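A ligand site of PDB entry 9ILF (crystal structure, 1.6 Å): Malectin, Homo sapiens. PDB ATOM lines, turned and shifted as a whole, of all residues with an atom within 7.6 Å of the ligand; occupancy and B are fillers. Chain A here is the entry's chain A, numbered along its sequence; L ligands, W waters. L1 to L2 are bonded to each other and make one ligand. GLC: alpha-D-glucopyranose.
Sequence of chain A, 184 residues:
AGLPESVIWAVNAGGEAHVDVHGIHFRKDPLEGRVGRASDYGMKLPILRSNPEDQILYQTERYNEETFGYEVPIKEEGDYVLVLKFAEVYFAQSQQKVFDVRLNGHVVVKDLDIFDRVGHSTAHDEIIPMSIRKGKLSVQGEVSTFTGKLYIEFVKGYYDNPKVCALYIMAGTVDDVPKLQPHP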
ATOM      1  N   ARG A  37      -7.791   5.083  30.082  1.00  0.00           N
ATOM      2  CA  ARG A  37      -6.867   5.326  28.968  1.00  0.00           C
ATOM      3  C   ARG A  37      -7.421   6.328  27.952  1.00  0.00           C
ATOM      4  O   ARG A  37      -8.500   6.110  27.380  1.00  0.00           O
ATOM      5  CB  ARG A  37      -6.557   4.002  28.238  1.00  0.00           C
ATOM      6  CG  ARG A  37      -6.182   2.841  29.160  1.00  0.00           C
ATOM      7  CD  ARG A  37      -5.884   1.558  28.381  1.00  0.00           C
ATOM      8  NE  ARG A  37      -5.475   0.459  29.260  1.00  0.00           N
ATOM      9  CZ  ARG A  37      -4.344   0.425  29.930  1.00  0.00           C
ATOM     10  NH1 ARG A  37      -3.397   1.347  29.750  1.00  0.00           N
ATOM     11  NH2 ARG A  37      -4.119  -0.565  30.794  1.00  0.00           N
ATOM     12  N   ALA A  38      -6.662   7.394  27.679  1.00  0.00           N
ATOM     13  CA  ALA A  38      -7.002   8.330  26.615  1.00  0.00           C
ATOM     14  C   ALA A  38      -6.601   7.802  25.230  1.00  0.00           C
ATOM     15  O   ALA A  38      -5.584   7.122  25.086  1.00  0.00           O
ATOM     16  CB  ALA A  38      -6.308   9.683  26.855  1.00  0.00           C
ATOM     17  N   SER A  39      -7.428   8.117  24.207  1.00  0.00           N
ATOM     18  CA  SER A  39      -7.083   7.794  22.815  1.00  0.00           C
ATOM     19  C   SER A  39      -7.543   8.880  21.839  1.00  0.00           C
ATOM     20  O   SER A  39      -8.713   9.274  21.838  1.00  0.00           O
ATOM     21  CB  SER A  39      -7.689   6.445  22.378  1.00  0.00           C
ATOM     22  OG  SER A  39      -7.445   6.257  20.968  1.00  0.00           O
ATOM     23  N   ASP A  40      -6.613   9.310  20.967  1.00  0.00           N
ATOM     24  CA  ASP A  40      -6.914  10.225  19.860  1.00  0.00           C
ATOM     25  C   ASP A  40      -6.957   9.509  18.504  1.00  0.00           C
ATOM     26  O   ASP A  40      -6.778  10.134  17.458  1.00  0.00           O
ATOM     27  CB  ASP A  40      -5.931  11.397  19.827  1.00  0.00           C
ATOM     28  CG  ASP A  40      -4.497  10.972  19.562  1.00  0.00           C
ATOM     29  OD1 ASP A  40      -3.634  11.869  19.442  1.00  0.00           O
ATOM     30  OD2 ASP A  40      -4.217   9.761  19.463  1.00  0.00           O
ATOM     31  N   TYR A  41      -7.251   8.196  18.507  1.00  0.00           N
ATOM     32  CA  TYR A  41      -7.320   7.407  17.264  1.00  0.00           C
ATOM     33  C   TYR A  41      -8.316   7.993  16.251  1.00  0.00           C
ATOM     34  O   TYR A  41      -8.069   7.943  15.042  1.00  0.00           O
ATOM     35  CB  TYR A  41      -7.673   5.937  17.593  1.00  0.00           C
ATOM     36  CG  TYR A  41      -7.731   5.007  16.368  1.00  0.00           C
ATOM     37  CD1 TYR A  41      -6.561   4.509  15.792  1.00  0.00           C
ATOM     38  CD2 TYR A  41      -8.950   4.677  15.779  1.00  0.00           C
ATOM     39  CE1 TYR A  41      -6.614   3.680  14.648  1.00  0.00           C
ATOM     40  CE2 TYR A  41      -9.003   3.848  14.635  1.00  0.00           C
ATOM     41  CZ  TYR A  41      -7.832   3.343  14.086  1.00  0.00           C
ATOM     42  OH  TYR A  41      -7.877   2.547  12.958  1.00  0.00           O
ATOM     43  N   GLY A  42      -9.444   8.531  16.712  1.00  0.00           N
ATOM     44  CA  GLY A  42     -10.461   9.071  15.804  1.00  0.00           C
ATOM     45  C   GLY A  42     -10.092  10.366  15.069  1.00  0.00           C
ATOM     46  O   GLY A  42     -10.876  10.798  14.204  1.00  0.00           O
ATOM     47  N   GLU A  61     -11.429  10.168  23.117  1.00  0.00           N
ATOM     48  CA  GLU A  61     -12.192   9.344  24.067  1.00  0.00           C
ATOM     49  C   GLU A  61     -11.350   8.979  25.303  1.00  0.00           C
ATOM     50  O   GLU A  61     -10.119   9.030  25.273  1.00  0.00           O
ATOM     51  CB  GLU A  61     -12.657   8.034  23.411  1.00  0.00           C
ATOM     52  CG  GLU A  61     -11.503   7.029  23.114  1.00  0.00           C
ATOM     53  CD  GLU A  61     -11.923   5.820  22.257  1.00  0.00           C
ATOM     54  OE1 GLU A  61     -12.590   4.899  22.789  1.00  0.00           O
ATOM     55  OE2 GLU A  61     -11.571   5.788  21.050  1.00  0.00           O
ATOM     56  N   ARG A  62     -12.049   8.564  26.372  1.00  0.00           N
ATOM     57  CA  ARG A  62     -11.480   7.745  27.453  1.00  0.00           C
ATOM     58  C   ARG A  62     -12.191   6.383  27.487  1.00  0.00           C
ATOM     59  O   ARG A  62     -13.426   6.335  27.453  1.00  0.00           O
ATOM     60  CB  ARG A  62     -11.577   8.465  28.827  1.00  0.00           C
ATOM     61  CG  ARG A  62     -10.889   7.721  30.004  1.00  0.00           C
ATOM     62  CD  ARG A  62     -10.618   8.648  31.240  1.00  0.00           C
ATOM     63  NE  ARG A  62      -9.681   9.709  30.897  1.00  0.00           N
ATOM     64  CZ  ARG A  62      -8.361   9.558  30.831  1.00  0.00           C
ATOM     65  NH1 ARG A  62      -7.771   8.457  31.262  1.00  0.00           N
ATOM     66  NH2 ARG A  62      -7.618  10.528  30.309  1.00  0.00           N
ATOM     67  N   TYR A  63     -11.417   5.290  27.554  1.00  0.00           N
ATOM     68  CA  TYR A  63     -11.952   3.916  27.619  1.00  0.00           C
ATOM     69  C   TYR A  63     -11.171   3.122  28.673  1.00  0.00           C
ATOM     70  O   TYR A  63     -10.133   3.574  29.171  1.00  0.00           O
ATOM     71  CB  TYR A  63     -11.905   3.208  26.248  1.00  0.00           C
ATOM     72  CG  TYR A  63     -10.531   2.707  25.799  1.00  0.00           C
ATOM     73  CD1 TYR A  63      -9.651   3.543  25.104  1.00  0.00           C
ATOM     74  CD2 TYR A  63     -10.124   1.397  26.044  1.00  0.00           C
ATOM     75  CE1 TYR A  63      -8.399   3.099  24.685  1.00  0.00           C
ATOM     76  CE2 TYR A  63      -8.867   0.946  25.631  1.00  0.00           C
ATOM     77  CZ  TYR A  63      -8.019   1.799  24.949  1.00  0.00           C
ATOM     78  OH  TYR A  63      -6.773   1.346  24.542  1.00  0.00           O
ATOM     79  N   ASN A  64     -11.660   1.912  29.024  1.00  0.00           N
ATOM     80  CA  ASN A  64     -10.955   1.070  29.995  1.00  0.00           C
ATOM     81  C   ASN A  64     -11.421  -0.389  29.878  1.00  0.00           C
ATOM     82  O   ASN A  64     -12.540  -0.668  29.445  1.00  0.00           O
ATOM     83  CB  ASN A  64     -11.185   1.574  31.436  1.00  0.00           C
ATOM     84  CG  ASN A  64     -10.062   1.174  32.405  1.00  0.00           C
ATOM     85  OD1 ASN A  64      -8.882   1.203  32.049  1.00  0.00           O
ATOM     86  ND2 ASN A  64     -10.442   0.834  33.631  1.00  0.00           N
ATOM     87  N   GLU A  65     -10.557  -1.327  30.307  1.00  0.00           N
ATOM     88  CA  GLU A  65     -10.901  -2.745  30.351  1.00  0.00           C
ATOM     89  C   GLU A  65     -11.558  -3.184  31.661  1.00  0.00           C
ATOM     90  O   GLU A  65     -11.947  -4.354  31.794  1.00  0.00           O
ATOM     91  CB  GLU A  65      -9.658  -3.592  30.061  1.00  0.00           C
ATOM     92  CG  GLU A  65      -8.533  -3.411  31.053  1.00  0.00           C
ATOM     93  CD  GLU A  65      -7.405  -2.538  30.494  1.00  0.00           C
ATOM     94  OE1 GLU A  65      -6.270  -3.051  30.380  1.00  0.00           O
ATOM     95  OE2 GLU A  65      -7.647  -1.329  30.199  1.00  0.00           O
ATOM     96  N   ALA A  87     -19.126   8.061  19.994  1.00  0.00           N
ATOM     97  CA  ALA A  87     -18.935   7.608  18.595  1.00  0.00           C
ATOM     98  C   ALA A  87     -18.144   6.294  18.594  1.00  0.00           C
ATOM     99  O   ALA A  87     -17.246   6.093  19.424  1.00  0.00           O
ATOM    100  CB  ALA A  87     -18.200   8.650  17.720  1.00  0.00           C
ATOM    101  N   GLU A  88     -18.454   5.402  17.614  1.00  0.00           N
ATOM    102  CA  GLU A  88     -17.717   4.145  17.423  1.00  0.00           C
ATOM    103  C   GLU A  88     -16.708   4.326  16.286  1.00  0.00           C
ATOM    104  O   GLU A  88     -17.084   4.372  15.103  1.00  0.00           O
ATOM    105  CB  GLU A  88     -18.691   2.986  17.140  1.00  0.00           C
ATOM    106  CG  GLU A  88     -18.010   1.614  16.857  1.00  0.00           C
ATOM    107  CD  GLU A  88     -17.140   1.115  17.995  1.00  0.00           C
ATOM    108  OE1 GLU A  88     -17.684   0.678  19.049  1.00  0.00           O
ATOM    109  OE2 GLU A  88     -15.890   1.155  17.845  1.00  0.00           O
ATOM    110  N   VAL A  89     -15.420   4.427  16.644  1.00  0.00           N
ATOM    111  CA  VAL A  89     -14.366   4.707  15.661  1.00  0.00           C
ATOM    112  C   VAL A  89     -13.535   3.467  15.320  1.00  0.00           C
ATOM    113  O   VAL A  89     -12.499   3.595  14.634  1.00  0.00           O
ATOM    114  CB  VAL A  89     -13.456   5.869  16.127  1.00  0.00           C
ATOM    115  CG1 VAL A  89     -14.269   7.184  16.311  1.00  0.00           C
ATOM    116  CG2 VAL A  89     -12.696   5.539  17.424  1.00  0.00           C
ATOM    117  N   TYR A  90     -13.944   2.266  15.773  1.00  0.00           N
ATOM    118  CA  TYR A  90     -13.199   1.025  15.470  1.00  0.00           C
ATOM    119  C   TYR A  90     -14.072  -0.041  14.800  1.00  0.00           C
ATOM    120  O   TYR A  90     -13.746  -0.480  13.678  1.00  0.00           O
ATOM    121  CB  TYR A  90     -12.527   0.448  16.738  1.00  0.00           C
ATOM    122  CG  TYR A  90     -11.487  -0.640  16.437  1.00  0.00           C
ATOM    123  CD1 TYR A  90     -10.255  -0.331  15.857  1.00  0.00           C
ATOM    124  CD2 TYR A  90     -11.738  -1.990  16.736  1.00  0.00           C
ATOM    125  CE1 TYR A  90      -9.302  -1.336  15.571  1.00  0.00           C
ATOM    126  CE2 TYR A  90     -10.786  -2.996  16.449  1.00  0.00           C
ATOM    127  CZ  TYR A  90      -9.587  -2.649  15.872  1.00  0.00           C
ATOM    128  OH  TYR A  90      -8.651  -3.651  15.586  1.00  0.00           O
ATOM    129  N   PHE A  91     -15.171  -0.485  15.425  1.00  0.00           N
ATOM    130  CA  PHE A  91     -16.019  -1.568  14.910  1.00  0.00           C
ATOM    131  C   PHE A  91     -17.083  -1.073  13.898  1.00  0.00           C
ATOM    132  O   PHE A  91     -17.432   0.113  13.847  1.00  0.00           O
ATOM    133  CB  PHE A  91     -16.713  -2.303  16.069  1.00  0.00           C
ATOM    134  CG  PHE A  91     -15.760  -3.009  17.011  1.00  0.00           C
ATOM    135  CD1 PHE A  91     -15.147  -4.210  16.654  1.00  0.00           C
ATOM    136  CD2 PHE A  91     -15.501  -2.492  18.280  1.00  0.00           C
ATOM    137  CE1 PHE A  91     -14.260  -4.870  17.528  1.00  0.00           C
ATOM    138  CE2 PHE A  91     -14.624  -3.142  19.156  1.00  0.00           C
ATOM    139  CZ  PHE A  91     -14.008  -4.326  18.781  1.00  0.00           C
ATOM    140  N   LYS A  97     -19.094  -4.105  20.623  1.00  0.00           N
ATOM    141  CA  LYS A  97     -18.910  -3.323  21.848  1.00  0.00           C
ATOM    142  C   LYS A  97     -20.285  -2.976  22.435  1.00  0.00           C
ATOM    143  O   LYS A  97     -21.078  -2.287  21.785  1.00  0.00           O
ATOM    144  CB  LYS A  97     -18.101  -2.038  21.583  1.00  0.00           C
ATOM    145  CG  LYS A  97     -17.897  -1.092  22.810  1.00  0.00           C
ATOM    146  CD  LYS A  97     -17.403   0.334  22.431  1.00  0.00           C
ATOM    147  CE  LYS A  97     -15.982   0.386  21.822  1.00  0.00           C
ATOM    148  NZ  LYS A  97     -14.916   0.058  22.838  1.00  0.00           N
ATOM    149  N   ASP A 160     -16.221  -6.229  24.450  1.00  0.00           N
ATOM    150  CA  ASP A 160     -15.180  -5.163  24.383  1.00  0.00           C
ATOM    151  C   ASP A 160     -15.282  -4.199  25.590  1.00  0.00           C
ATOM    152  O   ASP A 160     -15.740  -4.574  26.679  1.00  0.00           O
ATOM    153  CB  ASP A 160     -15.223  -4.472  23.014  1.00  0.00           C
ATOM    154  CG  ASP A 160     -13.864  -3.845  22.640  1.00  0.00           C
ATOM    155  OD1 ASP A 160     -12.941  -4.610  22.259  1.00  0.00           O
ATOM    156  OD2 ASP A 160     -13.696  -2.588  22.713  1.00  0.00           O
ATOM    157  N   ASN A 161     -14.796  -2.902  25.420  1.00  0.00           N
ATOM    158  CA  ASN A 161     -14.554  -1.961  26.536  1.00  0.00           C
ATOM    159  C   ASN A 161     -15.551  -0.792  26.594  1.00  0.00           C
ATOM    160  O   ASN A 161     -15.883  -0.196  25.557  1.00  0.00           O
ATOM    161  CB  ASN A 161     -13.130  -1.385  26.476  1.00  0.00           C
ATOM    162  CG  ASN A 161     -12.035  -2.477  26.391  1.00  0.00           C
ATOM    163  OD1 ASN A 161     -12.136  -3.513  27.068  1.00  0.00           O
ATOM    164  ND2 ASN A 161     -11.017  -2.253  25.569  1.00  0.00           N
ATOM    165  N   PRO A 162     -16.015  -0.413  27.799  1.00  0.00           N
ATOM    166  CA  PRO A 162     -16.805   0.835  27.952  1.00  0.00           C
ATOM    167  C   PRO A 162     -15.982   2.080  27.589  1.00  0.00           C
ATOM    168  O   PRO A 162     -14.764   2.113  27.779  1.00  0.00           O
ATOM    169  CB  PRO A 162     -17.207   0.820  29.431  1.00  0.00           C
ATOM    170  CG  PRO A 162     -16.082   0.023  30.093  1.00  0.00           C
ATOM    171  CD  PRO A 162     -15.797  -1.088  29.087  1.00  0.00           C
ATOM    172  N   LYS A 163     -16.676   3.117  27.079  1.00  0.00           N
ATOM    173  CA  LYS A 163     -16.012   4.349  26.621  1.00  0.00           C
ATOM    174  C   LYS A 163     -16.976   5.554  26.694  1.00  0.00           C
ATOM    175  O   LYS A 163     -18.194   5.383  26.783  1.00  0.00           O
ATOM    176  CB  LYS A 163     -15.484   4.197  25.172  1.00  0.00           C
ATOM    177  CG  LYS A 163     -16.593   4.176  24.073  1.00  0.00           C
ATOM    178  CD  LYS A 163     -16.031   4.307  22.633  1.00  0.00           C
ATOM    179  CE  LYS A 163     -15.670   5.747  22.260  1.00  0.00           C
ATOM    180  NZ  LYS A 163     -14.920   5.807  20.931  1.00  0.00           N
ATOM    181  N   VAL A 164     -16.409   6.773  26.664  1.00  0.00           N
ATOM    182  CA  VAL A 164     -17.175   8.027  26.535  1.00  0.00           C
ATOM    183  C   VAL A 164     -16.320   9.079  25.820  1.00  0.00           C
ATOM    184  O   VAL A 164     -15.096   9.101  25.957  1.00  0.00           O
ATOM    185  CB  VAL A 164     -17.683   8.524  27.921  1.00  0.00           C
ATOM    186  CG1 VAL A 164     -16.534   8.977  28.810  1.00  0.00           C
ATOM    187  CG2 VAL A 164     -18.723   9.651  27.765  1.00  0.00           C
HETATM  188  C1  GLC L   1      -7.682  -3.189  18.924  1.00  0.00           C
HETATM  189  C2  GLC L   1      -8.456  -1.954  19.335  1.00  0.00           C
HETATM  190  C3  GLC L   1      -9.123  -2.133  20.700  1.00  0.00           C
HETATM  191  C4  GLC L   1      -9.939  -3.402  20.722  1.00  0.00           C
HETATM  192  C5  GLC L   1      -9.132  -4.598  20.240  1.00  0.00           C
HETATM  193  C6  GLC L   1     -10.040  -5.805  20.111  1.00  0.00           C
HETATM  194  O1  GLC L   1      -6.534  -3.356  19.758  1.00  0.00           O
HETATM  195  O2  GLC L   1      -7.554  -0.830  19.313  1.00  0.00           O
HETATM  196  O3  GLC L   1     -10.075  -1.097  20.987  1.00  0.00           O
HETATM  197  O4  GLC L   1     -10.390  -3.640  22.062  1.00  0.00           O
HETATM  198  O5  GLC L   1      -8.533  -4.334  18.984  1.00  0.00           O
HETATM  199  O6  GLC L   1      -9.258  -6.996  20.015  1.00  0.00           O
HETATM  200  C1  GLC L   2      -9.683   0.039  21.835  1.00  0.00           C
HETATM  201  C2  GLC L   2     -10.915   0.647  22.525  1.00  0.00           C
HETATM  202  C3  GLC L   2     -11.766   1.473  21.553  1.00  0.00           C
HETATM  203  C4  GLC L   2     -10.880   2.501  20.853  1.00  0.00           C
HETATM  204  C5  GLC L   2      -9.686   1.792  20.197  1.00  0.00           C
HETATM  205  C6  GLC L   2      -8.719   2.735  19.469  1.00  0.00           C
HETATM  206  O2  GLC L   2     -11.662  -0.376  23.165  1.00  0.00           O
HETATM  207  O3  GLC L   2     -12.840   2.093  22.265  1.00  0.00           O
HETATM  208  O4  GLC L   2     -11.611   3.251  19.882  1.00  0.00           O
HETATM  209  O5  GLC L   2      -8.949   1.065  21.174  1.00  0.00           O
HETATM  210  O6  GLC L   2      -8.078   3.615  20.381  1.00  0.00           O
HETATM  211  O   HOH W   1      -5.924   2.536  21.969  1.00  0.00           O
HETATM  212  O   HOH W   2     -14.601   3.187  19.314  1.00  0.00           O
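OD1 of Asp 160 is in hydrogen-bond range of O4 of GLC L1, at 2.7 Å.
An oxygen (O3) of GLC L2 sits at hydrogen-bond distance from the side-chain amino group (NZ) of Lys 97, 3.0 Å away.
OE2 of Glu 61 is in hydrogen-bond range of O4 of GLC L2, at 2.8 Å.
The side-chain hydroxyl (OH) of Tyr 90 is in hydrogen-bond range of an oxygen (O5) of GLC L1 (3.5 Å).
OG of Ser 39 is in hydrogen-bond range of O6 of GLC L2, at 2.8 Å.
The side-chain amide nitrogen (ND2) of Asn 161 sits at hydrogen-bond distance from an oxygen (O2) of GLC L2, at 3.1 Å.
Merely in contact with the ligand: Val 89 (3.5 Å), Tyr 41 (3.7 Å), Tyr 63 (3.7 Å) and Lys 163 (3.9 Å).
Hydrophobic or aromatic side chains within 4 Å of the ligand: Tyr 41, Tyr 63, Val 89 and Tyr 90.
Within 4 Å of the ligand: Ser 39, Tyr 41, Glu 61, Tyr 63, Val 89, Tyr 90, Lys 97, Asp 160, Asn 161 and Lys 163.
The nearest printed residue that does not touch the ligand is Phe 91 (4.4 Å).
OD2 of Asp 160 lies within salt-bridge range of NZ of Lys 97, 2.9 Å away.
N of Tyr 90 sits at hydrogen-bond distance from OE2 of Glu 88 (3.1 Å).
OG of Ser 39 sits at hydrogen-bond distance from N of Tyr 41.
The backbone carbonyl oxygen of Tyr 63 lies within hydrogen-bond range of the backbone NH of Arg 37 (2.9 Å).
NZ of Lys 163 is in salt-bridge range of OE1 of Glu 61 (3.1 Å).
NZ of Lys 97 is in hydrogen-bond range of O of Asn 161.
N of Ser 39 is in hydrogen-bond range of O of Glu 61 (3.0 Å).
The backbone carbonyl oxygen (O) of Ala 87 sits at hydrogen-bond distance from the side-chain amino group (NZ) of Lys 163, 2.8 Å away.
Water W1 lies within hydrogen-bond range of an oxygen (O6) of GLC L2 (2.9 Å) and the side-chain hydroxyl (OH) of Tyr 63 (3.0 Å).
Water W2 lies within hydrogen-bond range of the side-chain carboxylate of Glu 88, an oxygen (O4) of GLC L2, the backbone NH of Val 89 and the side-chain amino group of Lys 163.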
